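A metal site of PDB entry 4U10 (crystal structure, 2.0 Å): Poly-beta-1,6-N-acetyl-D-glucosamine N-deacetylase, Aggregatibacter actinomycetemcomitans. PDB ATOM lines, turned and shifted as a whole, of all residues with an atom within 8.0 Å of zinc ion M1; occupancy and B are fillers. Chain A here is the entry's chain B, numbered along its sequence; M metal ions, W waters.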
ATOM      1  N   TYR A   9     -28.787 -15.423 -13.863  1.00  0.00           N
ATOM      2  CA  TYR A   9     -28.483 -16.868 -14.013  1.00  0.00           C
ATOM      3  C   TYR A   9     -26.999 -17.049 -14.378  1.00  0.00           C
ATOM      4  O   TYR A   9     -26.342 -16.088 -14.852  1.00  0.00           O
ATOM      5  CB  TYR A   9     -29.296 -17.506 -15.123  1.00  0.00           C
ATOM      6  CG  TYR A   9     -30.793 -17.584 -14.888  1.00  0.00           C
ATOM      7  CD1 TYR A   9     -31.353 -18.660 -14.207  1.00  0.00           C
ATOM      8  CD2 TYR A   9     -31.650 -16.597 -15.368  1.00  0.00           C
ATOM      9  CE1 TYR A   9     -32.707 -18.743 -14.004  1.00  0.00           C
ATOM     10  CE2 TYR A   9     -33.032 -16.666 -15.170  1.00  0.00           C
ATOM     11  CZ  TYR A   9     -33.550 -17.728 -14.489  1.00  0.00           C
ATOM     12  OH  TYR A   9     -34.918 -17.853 -14.281  1.00  0.00           O
ATOM     13  N   HIS A  10     -26.478 -18.248 -14.091  1.00  0.00           N
ATOM     14  CA  HIS A  10     -25.114 -18.590 -14.435  1.00  0.00           C
ATOM     15  C   HIS A  10     -25.153 -19.835 -15.314  1.00  0.00           C
ATOM     16  O   HIS A  10     -25.790 -19.767 -16.402  1.00  0.00           O
ATOM     17  CB  HIS A  10     -24.295 -18.716 -13.136  1.00  0.00           C
ATOM     18  CG  HIS A  10     -24.069 -17.389 -12.494  1.00  0.00           C
ATOM     19  ND1 HIS A  10     -25.044 -16.775 -11.731  1.00  0.00           N
ATOM     20  CD2 HIS A  10     -23.080 -16.491 -12.617  1.00  0.00           C
ATOM     21  CE1 HIS A  10     -24.620 -15.605 -11.338  1.00  0.00           C
ATOM     22  NE2 HIS A  10     -23.430 -15.397 -11.863  1.00  0.00           N
ATOM     23  N   PRO A  26     -20.519 -21.869  -9.258  1.00  0.00           N
ATOM     24  CA  PRO A  26     -21.489 -21.242  -8.334  1.00  0.00           C
ATOM     25  C   PRO A  26     -22.862 -20.965  -8.985  1.00  0.00           C
ATOM     26  O   PRO A  26     -22.881 -20.463 -10.054  1.00  0.00           O
ATOM     27  CB  PRO A  26     -20.775 -19.908  -7.955  1.00  0.00           C
ATOM     28  CG  PRO A  26     -19.356 -20.064  -8.296  1.00  0.00           C
ATOM     29  CD  PRO A  26     -19.312 -21.046  -9.490  1.00  0.00           C
ATOM     30  N   PHE A  73     -27.449 -13.789 -18.112  1.00  0.00           N
ATOM     31  CA  PHE A  73     -26.703 -15.026 -17.930  1.00  0.00           C
ATOM     32  C   PHE A  73     -25.201 -14.595 -17.889  1.00  0.00           C
ATOM     33  O   PHE A  73     -24.734 -13.888 -18.766  1.00  0.00           O
ATOM     34  CB  PHE A  73     -26.986 -16.058 -19.080  1.00  0.00           C
ATOM     35  CG  PHE A  73     -28.424 -16.500 -19.137  1.00  0.00           C
ATOM     36  CD1 PHE A  73     -29.368 -15.751 -19.836  1.00  0.00           C
ATOM     37  CD2 PHE A  73     -28.849 -17.626 -18.451  1.00  0.00           C
ATOM     38  CE1 PHE A  73     -30.672 -16.139 -19.874  1.00  0.00           C
ATOM     39  CE2 PHE A  73     -30.165 -17.977 -18.395  1.00  0.00           C
ATOM     40  CZ  PHE A  73     -31.094 -17.231 -19.113  1.00  0.00           C
ATOM     41  N   ASP A  74     -24.519 -14.949 -16.802  1.00  0.00           N
ATOM     42  CA  ASP A  74     -23.172 -14.587 -16.615  1.00  0.00           C
ATOM     43  C   ASP A  74     -22.179 -15.727 -16.884  1.00  0.00           C
ATOM     44  O   ASP A  74     -22.435 -16.917 -16.494  1.00  0.00           O
ATOM     45  CB  ASP A  74     -22.925 -14.153 -15.183  1.00  0.00           C
ATOM     46  CG  ASP A  74     -23.620 -12.826 -14.790  1.00  0.00           C
ATOM     47  OD1 ASP A  74     -24.376 -12.174 -15.554  1.00  0.00           O
ATOM     48  OD2 ASP A  74     -23.431 -12.450 -13.615  1.00  0.00           O
ATOM     49  N   ASP A  75     -21.064 -15.327 -17.496  1.00  0.00           N
ATOM     50  CA  ASP A  75     -19.731 -15.971 -17.415  1.00  0.00           C
ATOM     51  C   ASP A  75     -19.120 -16.455 -18.725  1.00  0.00           C
ATOM     52  O   ASP A  75     -17.909 -16.316 -18.934  1.00  0.00           O
ATOM     53  CB  ASP A  75     -19.644 -17.094 -16.329  1.00  0.00           C
ATOM     54  CG  ASP A  75     -19.736 -16.564 -14.920  1.00  0.00           C
ATOM     55  OD1 ASP A  75     -19.755 -15.347 -14.759  1.00  0.00           O
ATOM     56  OD2 ASP A  75     -19.761 -17.374 -13.933  1.00  0.00           O
ATOM     57  N   GLY A  76     -19.988 -16.955 -19.607  1.00  0.00           N
ATOM     58  CA  GLY A  76     -19.618 -17.495 -20.910  1.00  0.00           C
ATOM     59  C   GLY A  76     -19.597 -19.010 -21.051  1.00  0.00           C
ATOM     60  O   GLY A  76     -18.997 -19.522 -21.972  1.00  0.00           O
ATOM     61  N   TYR A  77     -20.242 -19.719 -20.141  1.00  0.00           N
ATOM     62  CA  TYR A  77     -20.278 -21.162 -20.155  1.00  0.00           C
ATOM     63  C   TYR A  77     -20.965 -21.687 -21.400  1.00  0.00           C
ATOM     64  O   TYR A  77     -21.983 -21.089 -21.843  1.00  0.00           O
ATOM     65  CB  TYR A  77     -21.016 -21.729 -18.949  1.00  0.00           C
ATOM     66  CG  TYR A  77     -20.472 -21.307 -17.633  1.00  0.00           C
ATOM     67  CD1 TYR A  77     -19.156 -21.546 -17.276  1.00  0.00           C
ATOM     68  CD2 TYR A  77     -21.278 -20.649 -16.737  1.00  0.00           C
ATOM     69  CE1 TYR A  77     -18.680 -21.149 -16.020  1.00  0.00           C
ATOM     70  CE2 TYR A  77     -20.858 -20.283 -15.499  1.00  0.00           C
ATOM     71  CZ  TYR A  77     -19.585 -20.534 -15.121  1.00  0.00           C
ATOM     72  OH  TYR A  77     -19.208 -20.067 -13.882  1.00  0.00           O
ATOM     73  N   ALA A  98     -23.249 -12.143 -20.601  1.00  0.00           N
ATOM     74  CA  ALA A  98     -22.056 -11.500 -20.194  1.00  0.00           C
ATOM     75  C   ALA A  98     -20.929 -12.496 -20.034  1.00  0.00           C
ATOM     76  O   ALA A  98     -20.665 -12.956 -18.929  1.00  0.00           O
ATOM     77  CB  ALA A  98     -22.273 -10.702 -18.897  1.00  0.00           C
ATOM     78  N   PRO A  99     -20.258 -12.816 -21.135  1.00  0.00           N
ATOM     79  CA  PRO A  99     -19.024 -13.601 -21.036  1.00  0.00           C
ATOM     80  C   PRO A  99     -17.776 -12.830 -20.637  1.00  0.00           C
ATOM     81  O   PRO A  99     -17.592 -11.664 -20.996  1.00  0.00           O
ATOM     82  CB  PRO A  99     -18.875 -14.146 -22.450  1.00  0.00           C
ATOM     83  CG  PRO A  99     -19.381 -13.022 -23.353  1.00  0.00           C
ATOM     84  CD  PRO A  99     -20.495 -12.348 -22.535  1.00  0.00           C
ATOM     85  N   VAL A 100     -16.870 -13.492 -19.884  1.00  0.00           N
ATOM     86  CA  VAL A 100     -15.546 -13.005 -19.688  1.00  0.00           C
ATOM     87  C   VAL A 100     -14.749 -13.105 -20.973  1.00  0.00           C
ATOM     88  O   VAL A 100     -14.536 -14.209 -21.529  1.00  0.00           O
ATOM     89  CB  VAL A 100     -14.848 -13.783 -18.560  1.00  0.00           C
ATOM     90  CG1 VAL A 100     -13.481 -13.185 -18.249  1.00  0.00           C
ATOM     91  CG2 VAL A 100     -15.708 -13.738 -17.300  1.00  0.00           C
ATOM     92  N   TRP A 103     -11.448 -15.226 -21.504  1.00  0.00           N
ATOM     93  CA  TRP A 103     -11.752 -16.640 -21.384  1.00  0.00           C
ATOM     94  C   TRP A 103     -12.152 -17.084 -22.750  1.00  0.00           C
ATOM     95  O   TRP A 103     -11.566 -18.033 -23.283  1.00  0.00           O
ATOM     96  CB  TRP A 103     -12.838 -16.910 -20.376  1.00  0.00           C
ATOM     97  CG  TRP A 103     -12.432 -16.652 -18.968  1.00  0.00           C
ATOM     98  CD1 TRP A 103     -11.196 -16.233 -18.532  1.00  0.00           C
ATOM     99  CD2 TRP A 103     -13.235 -16.774 -17.809  1.00  0.00           C
ATOM    100  NE1 TRP A 103     -11.217 -16.111 -17.203  1.00  0.00           N
ATOM    101  CE2 TRP A 103     -12.453 -16.463 -16.727  1.00  0.00           C
ATOM    102  CE3 TRP A 103     -14.559 -17.195 -17.569  1.00  0.00           C
ATOM    103  CZ2 TRP A 103     -12.931 -16.514 -15.442  1.00  0.00           C
ATOM    104  CZ3 TRP A 103     -15.020 -17.227 -16.347  1.00  0.00           C
ATOM    105  CH2 TRP A 103     -14.223 -16.890 -15.279  1.00  0.00           C
ATOM    106  N   TYR A 114      -8.124 -20.289 -13.492  1.00  0.00           N
ATOM    107  CA  TYR A 114      -9.337 -20.147 -12.721  1.00  0.00           C
ATOM    108  C   TYR A 114      -9.008 -20.427 -11.227  1.00  0.00           C
ATOM    109  O   TYR A 114      -8.977 -21.568 -10.761  1.00  0.00           O
ATOM    110  CB  TYR A 114     -10.343 -21.108 -13.269  1.00  0.00           C
ATOM    111  CG  TYR A 114     -11.748 -20.962 -12.773  1.00  0.00           C
ATOM    112  CD1 TYR A 114     -12.581 -20.004 -13.298  1.00  0.00           C
ATOM    113  CD2 TYR A 114     -12.265 -21.823 -11.831  1.00  0.00           C
ATOM    114  CE1 TYR A 114     -13.904 -19.879 -12.885  1.00  0.00           C
ATOM    115  CE2 TYR A 114     -13.590 -21.706 -11.377  1.00  0.00           C
ATOM    116  CZ  TYR A 114     -14.387 -20.718 -11.936  1.00  0.00           C
ATOM    117  OH  TYR A 114     -15.673 -20.550 -11.569  1.00  0.00           O
ATOM    118  N   HIS A 144     -18.284  -8.621 -18.920  1.00  0.00           N
ATOM    119  CA  HIS A 144     -18.085  -9.192 -17.617  1.00  0.00           C
ATOM    120  C   HIS A 144     -16.639  -9.101 -17.218  1.00  0.00           C
ATOM    121  O   HIS A 144     -16.173  -9.915 -16.430  1.00  0.00           O
ATOM    122  CB  HIS A 144     -18.552 -10.657 -17.628  1.00  0.00           C
ATOM    123  CG  HIS A 144     -19.033 -11.199 -16.322  1.00  0.00           C
ATOM    124  ND1 HIS A 144     -19.734 -10.470 -15.392  1.00  0.00           N
ATOM    125  CD2 HIS A 144     -18.994 -12.473 -15.843  1.00  0.00           C
ATOM    126  CE1 HIS A 144     -20.058 -11.260 -14.372  1.00  0.00           C
ATOM    127  NE2 HIS A 144     -19.644 -12.490 -14.654  1.00  0.00           N
ATOM    128  N   THR A 145     -15.970  -8.017 -17.641  1.00  0.00           N
ATOM    129  CA  THR A 145     -14.575  -7.717 -17.573  1.00  0.00           C
ATOM    130  C   THR A 145     -13.773  -8.601 -18.493  1.00  0.00           C
ATOM    131  O   THR A 145     -14.279  -9.631 -18.984  1.00  0.00           O
ATOM    132  CB  THR A 145     -13.976  -7.818 -16.126  1.00  0.00           C
ATOM    133  OG1 THR A 145     -13.745  -9.189 -15.794  1.00  0.00           O
ATOM    134  CG2 THR A 145     -14.886  -7.140 -15.106  1.00  0.00           C
ATOM    135  N   HIS A 149     -12.197 -11.389 -13.362  1.00  0.00           N
ATOM    136  CA  HIS A 149     -13.124 -12.302 -12.726  1.00  0.00           C
ATOM    137  C   HIS A 149     -12.435 -13.298 -11.825  1.00  0.00           C
ATOM    138  O   HIS A 149     -12.594 -14.536 -11.981  1.00  0.00           O
ATOM    139  CB  HIS A 149     -13.884 -13.110 -13.734  1.00  0.00           C
ATOM    140  CG  HIS A 149     -15.211 -13.600 -13.269  1.00  0.00           C
ATOM    141  ND1 HIS A 149     -15.371 -14.639 -12.362  1.00  0.00           N
ATOM    142  CD2 HIS A 149     -16.460 -13.297 -13.715  1.00  0.00           C
ATOM    143  CE1 HIS A 149     -16.679 -14.874 -12.213  1.00  0.00           C
ATOM    144  NE2 HIS A 149     -17.357 -14.046 -13.004  1.00  0.00           N
ATOM    145  N   VAL A 207     -21.572  -5.974 -16.487  1.00  0.00           N
ATOM    146  CA  VAL A 207     -22.080  -6.819 -15.447  1.00  0.00           C
ATOM    147  C   VAL A 207     -20.939  -7.168 -14.501  1.00  0.00           C
ATOM    148  O   VAL A 207     -19.930  -7.816 -14.912  1.00  0.00           O
ATOM    149  CB  VAL A 207     -22.635  -8.137 -16.035  1.00  0.00           C
ATOM    150  CG1 VAL A 207     -23.196  -9.006 -14.931  1.00  0.00           C
ATOM    151  CG2 VAL A 207     -23.660  -7.912 -17.167  1.00  0.00           C
ATOM    152  N   TRP A 208     -21.109  -6.857 -13.201  1.00  0.00           N
ATOM    153  CA  TRP A 208     -20.034  -7.094 -12.226  1.00  0.00           C
ATOM    154  C   TRP A 208     -19.899  -8.527 -11.797  1.00  0.00           C
ATOM    155  O   TRP A 208     -20.887  -9.172 -11.442  1.00  0.00           O
ATOM    156  CB  TRP A 208     -20.227  -6.240 -10.978  1.00  0.00           C
ATOM    157  CG  TRP A 208     -20.489  -4.774 -11.256  1.00  0.00           C
ATOM    158  CD1 TRP A 208     -21.627  -4.100 -10.988  1.00  0.00           C
ATOM    159  CD2 TRP A 208     -19.582  -3.828 -11.777  1.00  0.00           C
ATOM    160  NE1 TRP A 208     -21.495  -2.795 -11.332  1.00  0.00           N
ATOM    161  CE2 TRP A 208     -20.255  -2.608 -11.851  1.00  0.00           C
ATOM    162  CE3 TRP A 208     -18.269  -3.896 -12.280  1.00  0.00           C
ATOM    163  CZ2 TRP A 208     -19.641  -1.449 -12.340  1.00  0.00           C
ATOM    164  CZ3 TRP A 208     -17.685  -2.760 -12.737  1.00  0.00           C
ATOM    165  CH2 TRP A 208     -18.359  -1.563 -12.777  1.00  0.00           C
ATOM    166  N   PRO A 209     -18.665  -9.095 -11.896  1.00  0.00           N
ATOM    167  CA  PRO A 209     -18.425 -10.431 -11.316  1.00  0.00           C
ATOM    168  C   PRO A 209     -18.874 -10.406  -9.880  1.00  0.00           C
ATOM    169  O   PRO A 209     -18.606  -9.439  -9.156  1.00  0.00           O
ATOM    170  CB  PRO A 209     -16.904 -10.588 -11.409  1.00  0.00           C
ATOM    171  CG  PRO A 209     -16.473  -9.671 -12.486  1.00  0.00           C
ATOM    172  CD  PRO A 209     -17.516  -8.588 -12.646  1.00  0.00           C
ATOM    173  N   TYR A 210     -19.627 -11.467  -9.485  1.00  0.00           N
ATOM    174  CA  TYR A 210     -20.092 -11.704  -8.118  1.00  0.00           C
ATOM    175  C   TYR A 210     -20.955 -10.606  -7.592  1.00  0.00           C
ATOM    176  O   TYR A 210     -21.153 -10.563  -6.391  1.00  0.00           O
ATOM    177  CB  TYR A 210     -18.934 -11.862  -7.101  1.00  0.00           C
ATOM    178  CG  TYR A 210     -17.678 -12.507  -7.664  1.00  0.00           C
ATOM    179  CD1 TYR A 210     -17.642 -13.849  -8.016  1.00  0.00           C
ATOM    180  CD2 TYR A 210     -16.548 -11.747  -7.888  1.00  0.00           C
ATOM    181  CE1 TYR A 210     -16.500 -14.434  -8.563  1.00  0.00           C
ATOM    182  CE2 TYR A 210     -15.392 -12.304  -8.440  1.00  0.00           C
ATOM    183  CZ  TYR A 210     -15.379 -13.663  -8.760  1.00  0.00           C
ATOM    184  OH  TYR A 210     -14.202 -14.153  -9.301  1.00  0.00           O
ATOM    185  N   GLY A 211     -21.411  -9.698  -8.456  1.00  0.00           N
ATOM    186  CA  GLY A 211     -22.271  -8.594  -7.982  1.00  0.00           C
ATOM    187  C   GLY A 211     -21.495  -7.521  -7.231  1.00  0.00           C
ATOM    188  O   GLY A 211     -22.103  -6.590  -6.675  1.00  0.00           O
ATOM    189  N   ARG A 247     -30.371  -7.066  -9.624  1.00  0.00           N
ATOM    190  CA  ARG A 247     -30.822  -8.339 -10.164  1.00  0.00           C
ATOM    191  C   ARG A 247     -31.082  -9.373  -9.100  1.00  0.00           C
ATOM    192  O   ARG A 247     -30.437  -9.357  -8.066  1.00  0.00           O
ATOM    193  CB  ARG A 247     -29.753  -8.941 -11.108  1.00  0.00           C
ATOM    194  CG  ARG A 247     -29.187  -8.003 -12.191  1.00  0.00           C
ATOM    195  CD  ARG A 247     -28.270  -8.772 -13.196  1.00  0.00           C
ATOM    196  NE  ARG A 247     -27.012  -9.250 -12.588  1.00  0.00           N
ATOM    197  CZ  ARG A 247     -26.170 -10.135 -13.171  1.00  0.00           C
ATOM    198  NH1 ARG A 247     -26.477 -10.707 -14.359  1.00  0.00           N
ATOM    199  NH2 ARG A 247     -25.085 -10.508 -12.538  1.00  0.00           N
HETATM  200 ZN    ZN M   1     -19.425 -14.082 -13.290  1.00  0.00          ZN
HETATM  201 ZN    ZN M   2     -22.548 -13.526 -12.002  1.00  0.00          ZN
HETATM  202  O   HOH W   1     -19.352 -16.758 -11.286  1.00  0.00           O
HETATM  203  O   HOH W   2     -20.772 -13.708 -11.946  1.00  0.00           O
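Zinc ion M1 is bound by water W2 (1.9 Å), OD1 of Asp 75 (2.0 Å), NE2 of His 149 (2.1 Å) and NE2 of His 144 (2.1 Å). Zinc ion M1 has four donor atoms within binding distance.
O of Asp 75 is in hydrogen-bond range of N of Val 100 (3.2 Å). The backbone NH of Asp 75 is in hydrogen-bond range of the backbone carbonyl oxygen of Ala 98 (2.8 Å). OH of Tyr 77 lies within hydrogen-bond range of OD2 of Asp 75, 2.7 Å away. O of His 149 sits at hydrogen-bond distance from OH of Tyr 210, 3.1 Å away. A ring nitrogen (ND1) of His 144 is in hydrogen-bond range of the backbone carbonyl oxygen of Val 207 (2.7 Å). The side-chain carboxylate (OD1) of Asp 74 lies within salt-bridge range of the guanidinium group (NH1) of Arg 247. The backbone NH of Asp 74 lies within hydrogen-bond range of the backbone carbonyl oxygen of Tyr 9.
Merely in contact with zinc ion M1: Asp 74 (3.98 Å). Four residues have an atom within 4 Å of zinc ion M1: Asp 74, Asp 75, His 144 and His 149.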
